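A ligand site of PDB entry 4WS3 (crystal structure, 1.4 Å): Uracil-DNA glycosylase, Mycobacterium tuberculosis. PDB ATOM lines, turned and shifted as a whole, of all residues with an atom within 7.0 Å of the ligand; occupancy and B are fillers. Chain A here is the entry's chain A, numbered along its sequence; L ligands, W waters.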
ATOM      1  N   VAL A  76     -15.338 -12.112   2.459  1.00  0.00           N
ATOM      2  CA  VAL A  76     -14.220 -12.011   3.414  1.00  0.00           C
ATOM      3  C   VAL A  76     -14.750 -11.811   4.821  1.00  0.00           C
ATOM      4  O   VAL A  76     -15.501 -10.878   5.112  1.00  0.00           O
ATOM      5  CB  VAL A  76     -13.263 -10.848   3.086  1.00  0.00           C
ATOM      6  CG1 VAL A  76     -11.976 -11.052   3.889  1.00  0.00           C
ATOM      7  CG2 VAL A  76     -12.937 -10.794   1.614  1.00  0.00           C
ATOM      8  N   GLY A  77     -14.334 -12.723   5.693  1.00  0.00           N
ATOM      9  CA  GLY A  77     -14.542 -12.580   7.121  1.00  0.00           C
ATOM     10  C   GLY A  77     -13.237 -12.209   7.814  1.00  0.00           C
ATOM     11  O   GLY A  77     -12.210 -11.928   7.163  1.00  0.00           O
ATOM     12  N   GLN A  78     -13.284 -12.230   9.146  1.00  0.00           N
ATOM     13  CA  GLN A  78     -12.177 -11.759   9.959  1.00  0.00           C
ATOM     14  C   GLN A  78     -11.321 -12.928  10.476  1.00  0.00           C
ATOM     15  O   GLN A  78     -10.212 -13.134  10.008  1.00  0.00           O
ATOM     16  CB  GLN A  78     -12.696 -10.838  11.047  1.00  0.00           C
ATOM     17  CG  GLN A  78     -11.602 -10.034  11.717  1.00  0.00           C
ATOM     18  CD  GLN A  78     -10.834  -9.177  10.736  1.00  0.00           C
ATOM     19  OE1 GLN A  78     -11.449  -8.418   9.963  1.00  0.00           O
ATOM     20  NE2 GLN A  78      -9.516  -9.318  10.720  1.00  0.00           N
ATOM     21  N   ASP A  79     -11.894 -13.652  11.427  1.00  0.00           N
ATOM     22  CA  ASP A  79     -11.235 -14.758  12.129  1.00  0.00           C
ATOM     23  C   ASP A  79     -12.151 -16.016  12.055  1.00  0.00           C
ATOM     24  O   ASP A  79     -13.367 -15.871  11.873  1.00  0.00           O
ATOM     25  CB  ASP A  79     -10.949 -14.382  13.586  1.00  0.00           C
ATOM     26  CG  ASP A  79     -10.003 -13.175  13.736  1.00  0.00           C
ATOM     27  OD1 ASP A  79      -8.779 -13.319  13.572  1.00  0.00           O
ATOM     28  OD2 ASP A  79     -10.503 -12.100  14.053  1.00  0.00           O
ATOM     29  N   PRO A  80     -11.589 -17.237  12.146  1.00  0.00           N
ATOM     30  CA  PRO A  80     -12.489 -18.389  12.208  1.00  0.00           C
ATOM     31  C   PRO A  80     -13.343 -18.421  13.472  1.00  0.00           C
ATOM     32  O   PRO A  80     -13.012 -17.783  14.474  1.00  0.00           O
ATOM     33  CB  PRO A  80     -11.554 -19.594  12.189  1.00  0.00           C
ATOM     34  CG  PRO A  80     -10.256 -19.041  11.619  1.00  0.00           C
ATOM     35  CD  PRO A  80     -10.180 -17.667  12.171  1.00  0.00           C
ATOM     36  N   TYR A  81     -14.435 -19.166  13.433  1.00  0.00           N
ATOM     37  CA  TYR A  81     -15.210 -19.421  14.642  1.00  0.00           C
ATOM     38  C   TYR A  81     -14.270 -19.904  15.755  1.00  0.00           C
ATOM     39  O   TYR A  81     -13.450 -20.773  15.525  1.00  0.00           O
ATOM     40  CB  TYR A  81     -16.228 -20.494  14.421  1.00  0.00           C
ATOM     41  CG  TYR A  81     -17.372 -20.144  13.534  1.00  0.00           C
ATOM     42  CD1 TYR A  81     -18.344 -19.203  13.913  1.00  0.00           C
ATOM     43  CD2 TYR A  81     -17.540 -20.794  12.293  1.00  0.00           C
ATOM     44  CE1 TYR A  81     -19.418 -18.897  13.102  1.00  0.00           C
ATOM     45  CE2 TYR A  81     -18.627 -20.517  11.483  1.00  0.00           C
ATOM     46  CZ  TYR A  81     -19.564 -19.583  11.889  1.00  0.00           C
ATOM     47  OH  TYR A  81     -20.670 -19.255  11.097  1.00  0.00           O
ATOM     48  N   PRO A  82     -14.444 -19.362  16.972  1.00  0.00           N
ATOM     49  CA  PRO A  82     -13.622 -19.777  18.095  1.00  0.00           C
ATOM     50  C   PRO A  82     -14.105 -20.987  18.881  1.00  0.00           C
ATOM     51  O   PRO A  82     -13.361 -21.466  19.763  1.00  0.00           O
ATOM     52  CB  PRO A  82     -13.625 -18.525  18.979  1.00  0.00           C
ATOM     53  CG  PRO A  82     -14.947 -17.912  18.756  1.00  0.00           C
ATOM     54  CD  PRO A  82     -15.257 -18.188  17.284  1.00  0.00           C
ATOM     55  N   ALA A  87     -15.291 -24.129  13.132  1.00  0.00           N
ATOM     56  CA  ALA A  87     -14.506 -23.709  11.970  1.00  0.00           C
ATOM     57  C   ALA A  87     -14.094 -24.919  11.117  1.00  0.00           C
ATOM     58  O   ALA A  87     -13.602 -25.936  11.626  1.00  0.00           O
ATOM     59  CB  ALA A  87     -13.258 -22.975  12.405  1.00  0.00           C
ATOM     60  N   LEU A  90     -13.631 -22.710   5.639  1.00  0.00           N
ATOM     61  CA  LEU A  90     -14.374 -21.853   4.746  1.00  0.00           C
ATOM     62  C   LEU A  90     -15.049 -20.865   5.643  1.00  0.00           C
ATOM     63  O   LEU A  90     -15.756 -21.259   6.585  1.00  0.00           O
ATOM     64  CB  LEU A  90     -15.404 -22.676   3.961  1.00  0.00           C
ATOM     65  CG  LEU A  90     -14.869 -23.735   2.996  1.00  0.00           C
ATOM     66  CD1 LEU A  90     -16.066 -24.435   2.357  1.00  0.00           C
ATOM     67  CD2 LEU A  90     -13.902 -23.158   1.960  1.00  0.00           C
ATOM     68  N   SER A  91     -14.852 -19.579   5.380  1.00  0.00           N
ATOM     69  CA  SER A  91     -15.434 -18.571   6.257  1.00  0.00           C
ATOM     70  C   SER A  91     -16.965 -18.776   6.420  1.00  0.00           C
ATOM     71  O   SER A  91     -17.670 -19.082   5.474  1.00  0.00           O
ATOM     72  CB  SER A  91     -15.066 -17.172   5.815  1.00  0.00           C
ATOM     73  OG  SER A  91     -15.644 -16.865   4.554  1.00  0.00           O
ATOM     74  N   PHE A  92     -17.407 -18.660   7.677  1.00  0.00           N
ATOM     75  CA  PHE A  92     -18.804 -18.758   8.102  1.00  0.00           C
ATOM     76  C   PHE A  92     -19.455 -20.138   8.024  1.00  0.00           C
ATOM     77  O   PHE A  92     -20.503 -20.345   8.646  1.00  0.00           O
ATOM     78  CB  PHE A  92     -19.698 -17.720   7.394  1.00  0.00           C
ATOM     79  CG  PHE A  92     -19.204 -16.325   7.590  1.00  0.00           C
ATOM     80  CD1 PHE A  92     -19.493 -15.633   8.776  1.00  0.00           C
ATOM     81  CD2 PHE A  92     -18.388 -15.720   6.643  1.00  0.00           C
ATOM     82  CE1 PHE A  92     -19.010 -14.373   8.988  1.00  0.00           C
ATOM     83  CE2 PHE A  92     -17.897 -14.445   6.880  1.00  0.00           C
ATOM     84  CZ  PHE A  92     -18.206 -13.770   8.035  1.00  0.00           C
ATOM     85  N   SER A  93     -18.828 -21.095   7.321  1.00  0.00           N
ATOM     86  CA  SER A  93     -19.417 -22.414   7.123  1.00  0.00           C
ATOM     87  C   SER A  93     -19.297 -23.294   8.365  1.00  0.00           C
ATOM     88  O   SER A  93     -18.389 -23.105   9.186  1.00  0.00           O
ATOM     89  CB  SER A  93     -18.664 -23.113   5.984  1.00  0.00           C
ATOM     90  OG  SER A  93     -19.332 -24.268   5.511  1.00  0.00           O
ATOM     91  N   PRO A 102     -24.226 -21.488  14.332  1.00  0.00           N
ATOM     92  CA  PRO A 102     -23.749 -20.240  14.946  1.00  0.00           C
ATOM     93  C   PRO A 102     -24.611 -19.055  14.518  1.00  0.00           C
ATOM     94  O   PRO A 102     -25.158 -19.029  13.381  1.00  0.00           O
ATOM     95  CB  PRO A 102     -22.331 -20.084  14.387  1.00  0.00           C
ATOM     96  CG  PRO A 102     -21.933 -21.437  13.903  1.00  0.00           C
ATOM     97  CD  PRO A 102     -23.184 -22.168  13.540  1.00  0.00           C
ATOM     98  N   SER A 104     -23.957 -16.049  13.492  1.00  0.00           N
ATOM     99  CA  SER A 104     -23.612 -15.339  12.258  1.00  0.00           C
ATOM    100  C   SER A 104     -24.215 -16.064  11.081  1.00  0.00           C
ATOM    101  O   SER A 104     -24.688 -15.413  10.116  1.00  0.00           O
ATOM    102  CB  SER A 104     -22.087 -15.217  12.071  1.00  0.00           C
ATOM    103  OG  SER A 104     -21.503 -14.283  12.958  1.00  0.00           O
ATOM    104  N   LEU A 105     -24.096 -17.392  11.080  1.00  0.00           N
ATOM    105  CA  LEU A 105     -24.606 -18.195   9.993  1.00  0.00           C
ATOM    106  C   LEU A 105     -26.125 -18.188   9.924  1.00  0.00           C
ATOM    107  O   LEU A 105     -26.696 -18.112   8.841  1.00  0.00           O
ATOM    108  CB  LEU A 105     -24.041 -19.601  10.091  1.00  0.00           C
ATOM    109  CG  LEU A 105     -24.320 -20.552   8.923  1.00  0.00           C
ATOM    110  CD1 LEU A 105     -23.808 -20.023   7.590  1.00  0.00           C
ATOM    111  CD2 LEU A 105     -23.716 -21.915   9.194  1.00  0.00           C
ATOM    112  N   LEU A 136     -14.567 -18.277   0.140  1.00  0.00           N
ATOM    113  CA  LEU A 136     -15.014 -18.006   1.500  1.00  0.00           C
ATOM    114  C   LEU A 136     -13.761 -17.810   2.398  1.00  0.00           C
ATOM    115  O   LEU A 136     -13.303 -18.737   3.078  1.00  0.00           O
ATOM    116  CB  LEU A 136     -15.904 -19.138   2.012  1.00  0.00           C
ATOM    117  CG  LEU A 136     -17.250 -19.234   1.268  1.00  0.00           C
ATOM    118  CD1 LEU A 136     -17.887 -20.597   1.480  1.00  0.00           C
ATOM    119  CD2 LEU A 136     -18.186 -18.116   1.731  1.00  0.00           C
ATOM    120  N   LEU A 137     -13.230 -16.608   2.337  1.00  0.00           N
ATOM    121  CA  LEU A 137     -11.932 -16.273   2.900  1.00  0.00           C
ATOM    122  C   LEU A 137     -12.088 -15.615   4.262  1.00  0.00           C
ATOM    123  O   LEU A 137     -13.001 -14.851   4.482  1.00  0.00           O
ATOM    124  CB  LEU A 137     -11.203 -15.316   1.969  1.00  0.00           C
ATOM    125  CG  LEU A 137      -9.747 -14.981   2.310  1.00  0.00           C
ATOM    126  CD1 LEU A 137      -8.880 -16.231   2.263  1.00  0.00           C
ATOM    127  CD2 LEU A 137      -9.298 -13.889   1.307  1.00  0.00           C
ATOM    128  N   ASN A 138     -11.253 -15.961   5.218  1.00  0.00           N
ATOM    129  CA  ASN A 138     -11.068 -15.142   6.384  1.00  0.00           C
ATOM    130  C   ASN A 138      -9.702 -14.450   6.273  1.00  0.00           C
ATOM    131  O   ASN A 138      -8.777 -15.011   5.712  1.00  0.00           O
ATOM    132  CB  ASN A 138     -11.066 -15.996   7.650  1.00  0.00           C
ATOM    133  CG  ASN A 138     -12.454 -16.298   8.157  1.00  0.00           C
ATOM    134  OD1 ASN A 138     -13.310 -15.407   8.205  1.00  0.00           O
ATOM    135  ND2 ASN A 138     -12.688 -17.540   8.567  1.00  0.00           N
ATOM    136  N   ARG A 139      -9.596 -13.254   6.810  1.00  0.00           N
ATOM    137  CA  ARG A 139      -8.307 -12.566   6.787  1.00  0.00           C
ATOM    138  C   ARG A 139      -7.231 -13.287   7.588  1.00  0.00           C
ATOM    139  O   ARG A 139      -6.037 -13.267   7.219  1.00  0.00           O
ATOM    140  CB  ARG A 139      -8.482 -11.141   7.243  1.00  0.00           C
ATOM    141  CG  ARG A 139      -9.068 -10.296   6.132  1.00  0.00           C
ATOM    142  CD  ARG A 139      -7.948  -9.872   5.190  1.00  0.00           C
ATOM    143  NE  ARG A 139      -7.105  -8.846   5.826  1.00  0.00           N
ATOM    144  CZ  ARG A 139      -5.797  -8.678   5.642  1.00  0.00           C
ATOM    145  NH1 ARG A 139      -5.079  -9.476   4.867  1.00  0.00           N
ATOM    146  NH2 ARG A 139      -5.171  -7.698   6.277  1.00  0.00           N
ATOM    147  N   TRP A 179     -17.504  -8.904   5.082  1.00  0.00           N
ATOM    148  CA  TRP A 179     -18.278  -9.237   6.283  1.00  0.00           C
ATOM    149  C   TRP A 179     -17.430  -9.271   7.560  1.00  0.00           C
ATOM    150  O   TRP A 179     -17.866  -9.842   8.558  1.00  0.00           O
ATOM    151  CB  TRP A 179     -18.966 -10.580   6.091  1.00  0.00           C
ATOM    152  CG  TRP A 179     -20.188 -10.553   5.258  1.00  0.00           C
ATOM    153  CD1 TRP A 179     -20.876  -9.439   4.796  1.00  0.00           C
ATOM    154  CD2 TRP A 179     -20.915 -11.695   4.753  1.00  0.00           C
ATOM    155  NE1 TRP A 179     -21.959  -9.839   4.061  1.00  0.00           N
ATOM    156  CE2 TRP A 179     -22.017 -11.211   4.021  1.00  0.00           C
ATOM    157  CE3 TRP A 179     -20.747 -13.085   4.882  1.00  0.00           C
ATOM    158  CZ2 TRP A 179     -22.915 -12.066   3.399  1.00  0.00           C
ATOM    159  CZ3 TRP A 179     -21.645 -13.936   4.246  1.00  0.00           C
ATOM    160  CH2 TRP A 179     -22.717 -13.412   3.507  1.00  0.00           C
ATOM    161  N   GLY A 180     -16.236  -8.707   7.494  1.00  0.00           N
ATOM    162  CA  GLY A 180     -15.295  -8.598   8.631  1.00  0.00           C
ATOM    163  C   GLY A 180     -15.055  -7.183   9.077  1.00  0.00           C
ATOM    164  O   GLY A 180     -15.447  -6.219   8.402  1.00  0.00           O
ATOM    165  N   ARG A 181     -14.368  -7.048  10.198  1.00  0.00           N
ATOM    166  CA  ARG A 181     -14.169  -5.755  10.874  1.00  0.00           C
ATOM    167  C   ARG A 181     -13.271  -4.873  10.045  1.00  0.00           C
ATOM    168  O   ARG A 181     -13.426  -3.653  10.011  1.00  0.00           O
ATOM    169  CB  ARG A 181     -13.545  -5.965  12.268  1.00  0.00           C
ATOM    170  N   PRO A 205     -22.717  -9.932   9.399  1.00  0.00           N
ATOM    171  CA  PRO A 205     -23.884 -10.700   9.770  1.00  0.00           C
ATOM    172  C   PRO A 205     -24.460 -10.339  11.138  1.00  0.00           C
ATOM    173  O   PRO A 205     -25.694 -10.262  11.283  1.00  0.00           O
ATOM    174  CB  PRO A 205     -23.370 -12.154   9.701  1.00  0.00           C
ATOM    175  CG  PRO A 205     -22.393 -12.099   8.561  1.00  0.00           C
ATOM    176  CD  PRO A 205     -21.707 -10.759   8.703  1.00  0.00           C
ATOM    177  N   LEU A 206     -23.598 -10.046  12.105  1.00  0.00           N
ATOM    178  CA  LEU A 206     -24.079  -9.731  13.439  1.00  0.00           C
ATOM    179  C   LEU A 206     -24.710  -8.335  13.565  1.00  0.00           C
ATOM    180  O   LEU A 206     -25.336  -8.077  14.561  1.00  0.00           O
ATOM    181  CB  LEU A 206     -23.012  -9.946  14.514  1.00  0.00           C
ATOM    182  CG  LEU A 206     -22.549 -11.412  14.603  1.00  0.00           C
ATOM    183  CD1 LEU A 206     -21.454 -11.516  15.656  1.00  0.00           C
ATOM    184  CD2 LEU A 206     -23.703 -12.338  14.928  1.00  0.00           C
HETATM  185  O1  LIG L   1     -15.503 -13.353  10.340  1.00  0.00           O
HETATM  186  C1  LIG L   1     -15.956 -14.479  10.651  1.00  0.00           C
HETATM  187  N1  LIG L   1     -15.541 -15.557   9.990  1.00  0.00           N
HETATM  188  C2  LIG L   1     -15.930 -16.788  10.307  1.00  0.00           C
HETATM  189  O2  LIG L   1     -15.454 -17.800   9.650  1.00  0.00           O
HETATM  190  N2  LIG L   1     -16.851 -14.612  11.637  1.00  0.00           N
HETATM  191  C3  LIG L   1     -17.314 -15.837  11.964  1.00  0.00           C
HETATM  192  N3  LIG L   1     -18.264 -15.925  12.946  1.00  0.00           N
HETATM  193  C4  LIG L   1     -16.861 -16.971  11.298  1.00  0.00           C
HETATM  194  O   HOH W   1     -16.927 -10.816  10.879  1.00  0.00           O
HETATM  195  O   HOH W   2     -17.809 -12.587  13.724  1.00  0.00           O
HETATM  196  O   HOH W   3     -17.222 -16.045  15.851  1.00  0.00           O
HETATM  197  O   HOH W   4     -14.690 -20.279  10.609  1.00  0.00           O
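Water W4 bridges O2 of the ligand (2.8 Å) and N of Tyr 81 (3.0 Å).
Water W1 bridges O of Trp 179 (2.7 Å) and O1 of the ligand (3.0 Å).
Merely in contact with the ligand: Gly 77 (3.4 Å), Pro 80 (3.96 Å), Tyr 81 (3.2 Å), Ser 91 (3.5 Å) and Ser 104 (3.6 Å).
Hydrophobic or aromatic side chains within 4 Å of the ligand: Tyr 81 and Phe 92.
The backbone carbonyl oxygen (O) of Gln 78 sits at hydrogen-bond distance from the backbone NH (N) of Arg 139, at 3.3 Å.
The side-chain hydroxyl (OH) of Tyr 81 is in hydrogen-bond range of the backbone carbonyl oxygen (O) of Phe 92.
N of Ser 91 lies within hydrogen-bond range of O of Leu 136, at 2.9 Å.
O of Gly 77 is in hydrogen-bond range of N of Arg 139, at 3.0 Å.
OG of Ser 91 is in hydrogen-bond range of N of Leu 137 (3.3 Å).
The side-chain amide oxygen (OD1) of Asn 138 lies within hydrogen-bond range of the backbone NH (N) of Gln 78, 3.3 Å away.
OE1 of Gln 78 is in hydrogen-bond range of N of Arg 181, 3.2 Å away.
O of Leu 137 is in hydrogen-bond range of N of Gly 77, at 2.8 Å.
O of Asp 79 is in hydrogen-bond range of N1 of the ligand (2.9 Å).
The side-chain amide oxygen (OD1) of Asn 138 is in hydrogen-bond range of a nitrogen (N1) of the ligand, at 2.9 Å.
O2 of the ligand is in hydrogen-bond range of N of Phe 92, at 2.9 Å.
The backbone NH of Gln 78 lies within hydrogen-bond range of an oxygen (O1) of the ligand.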
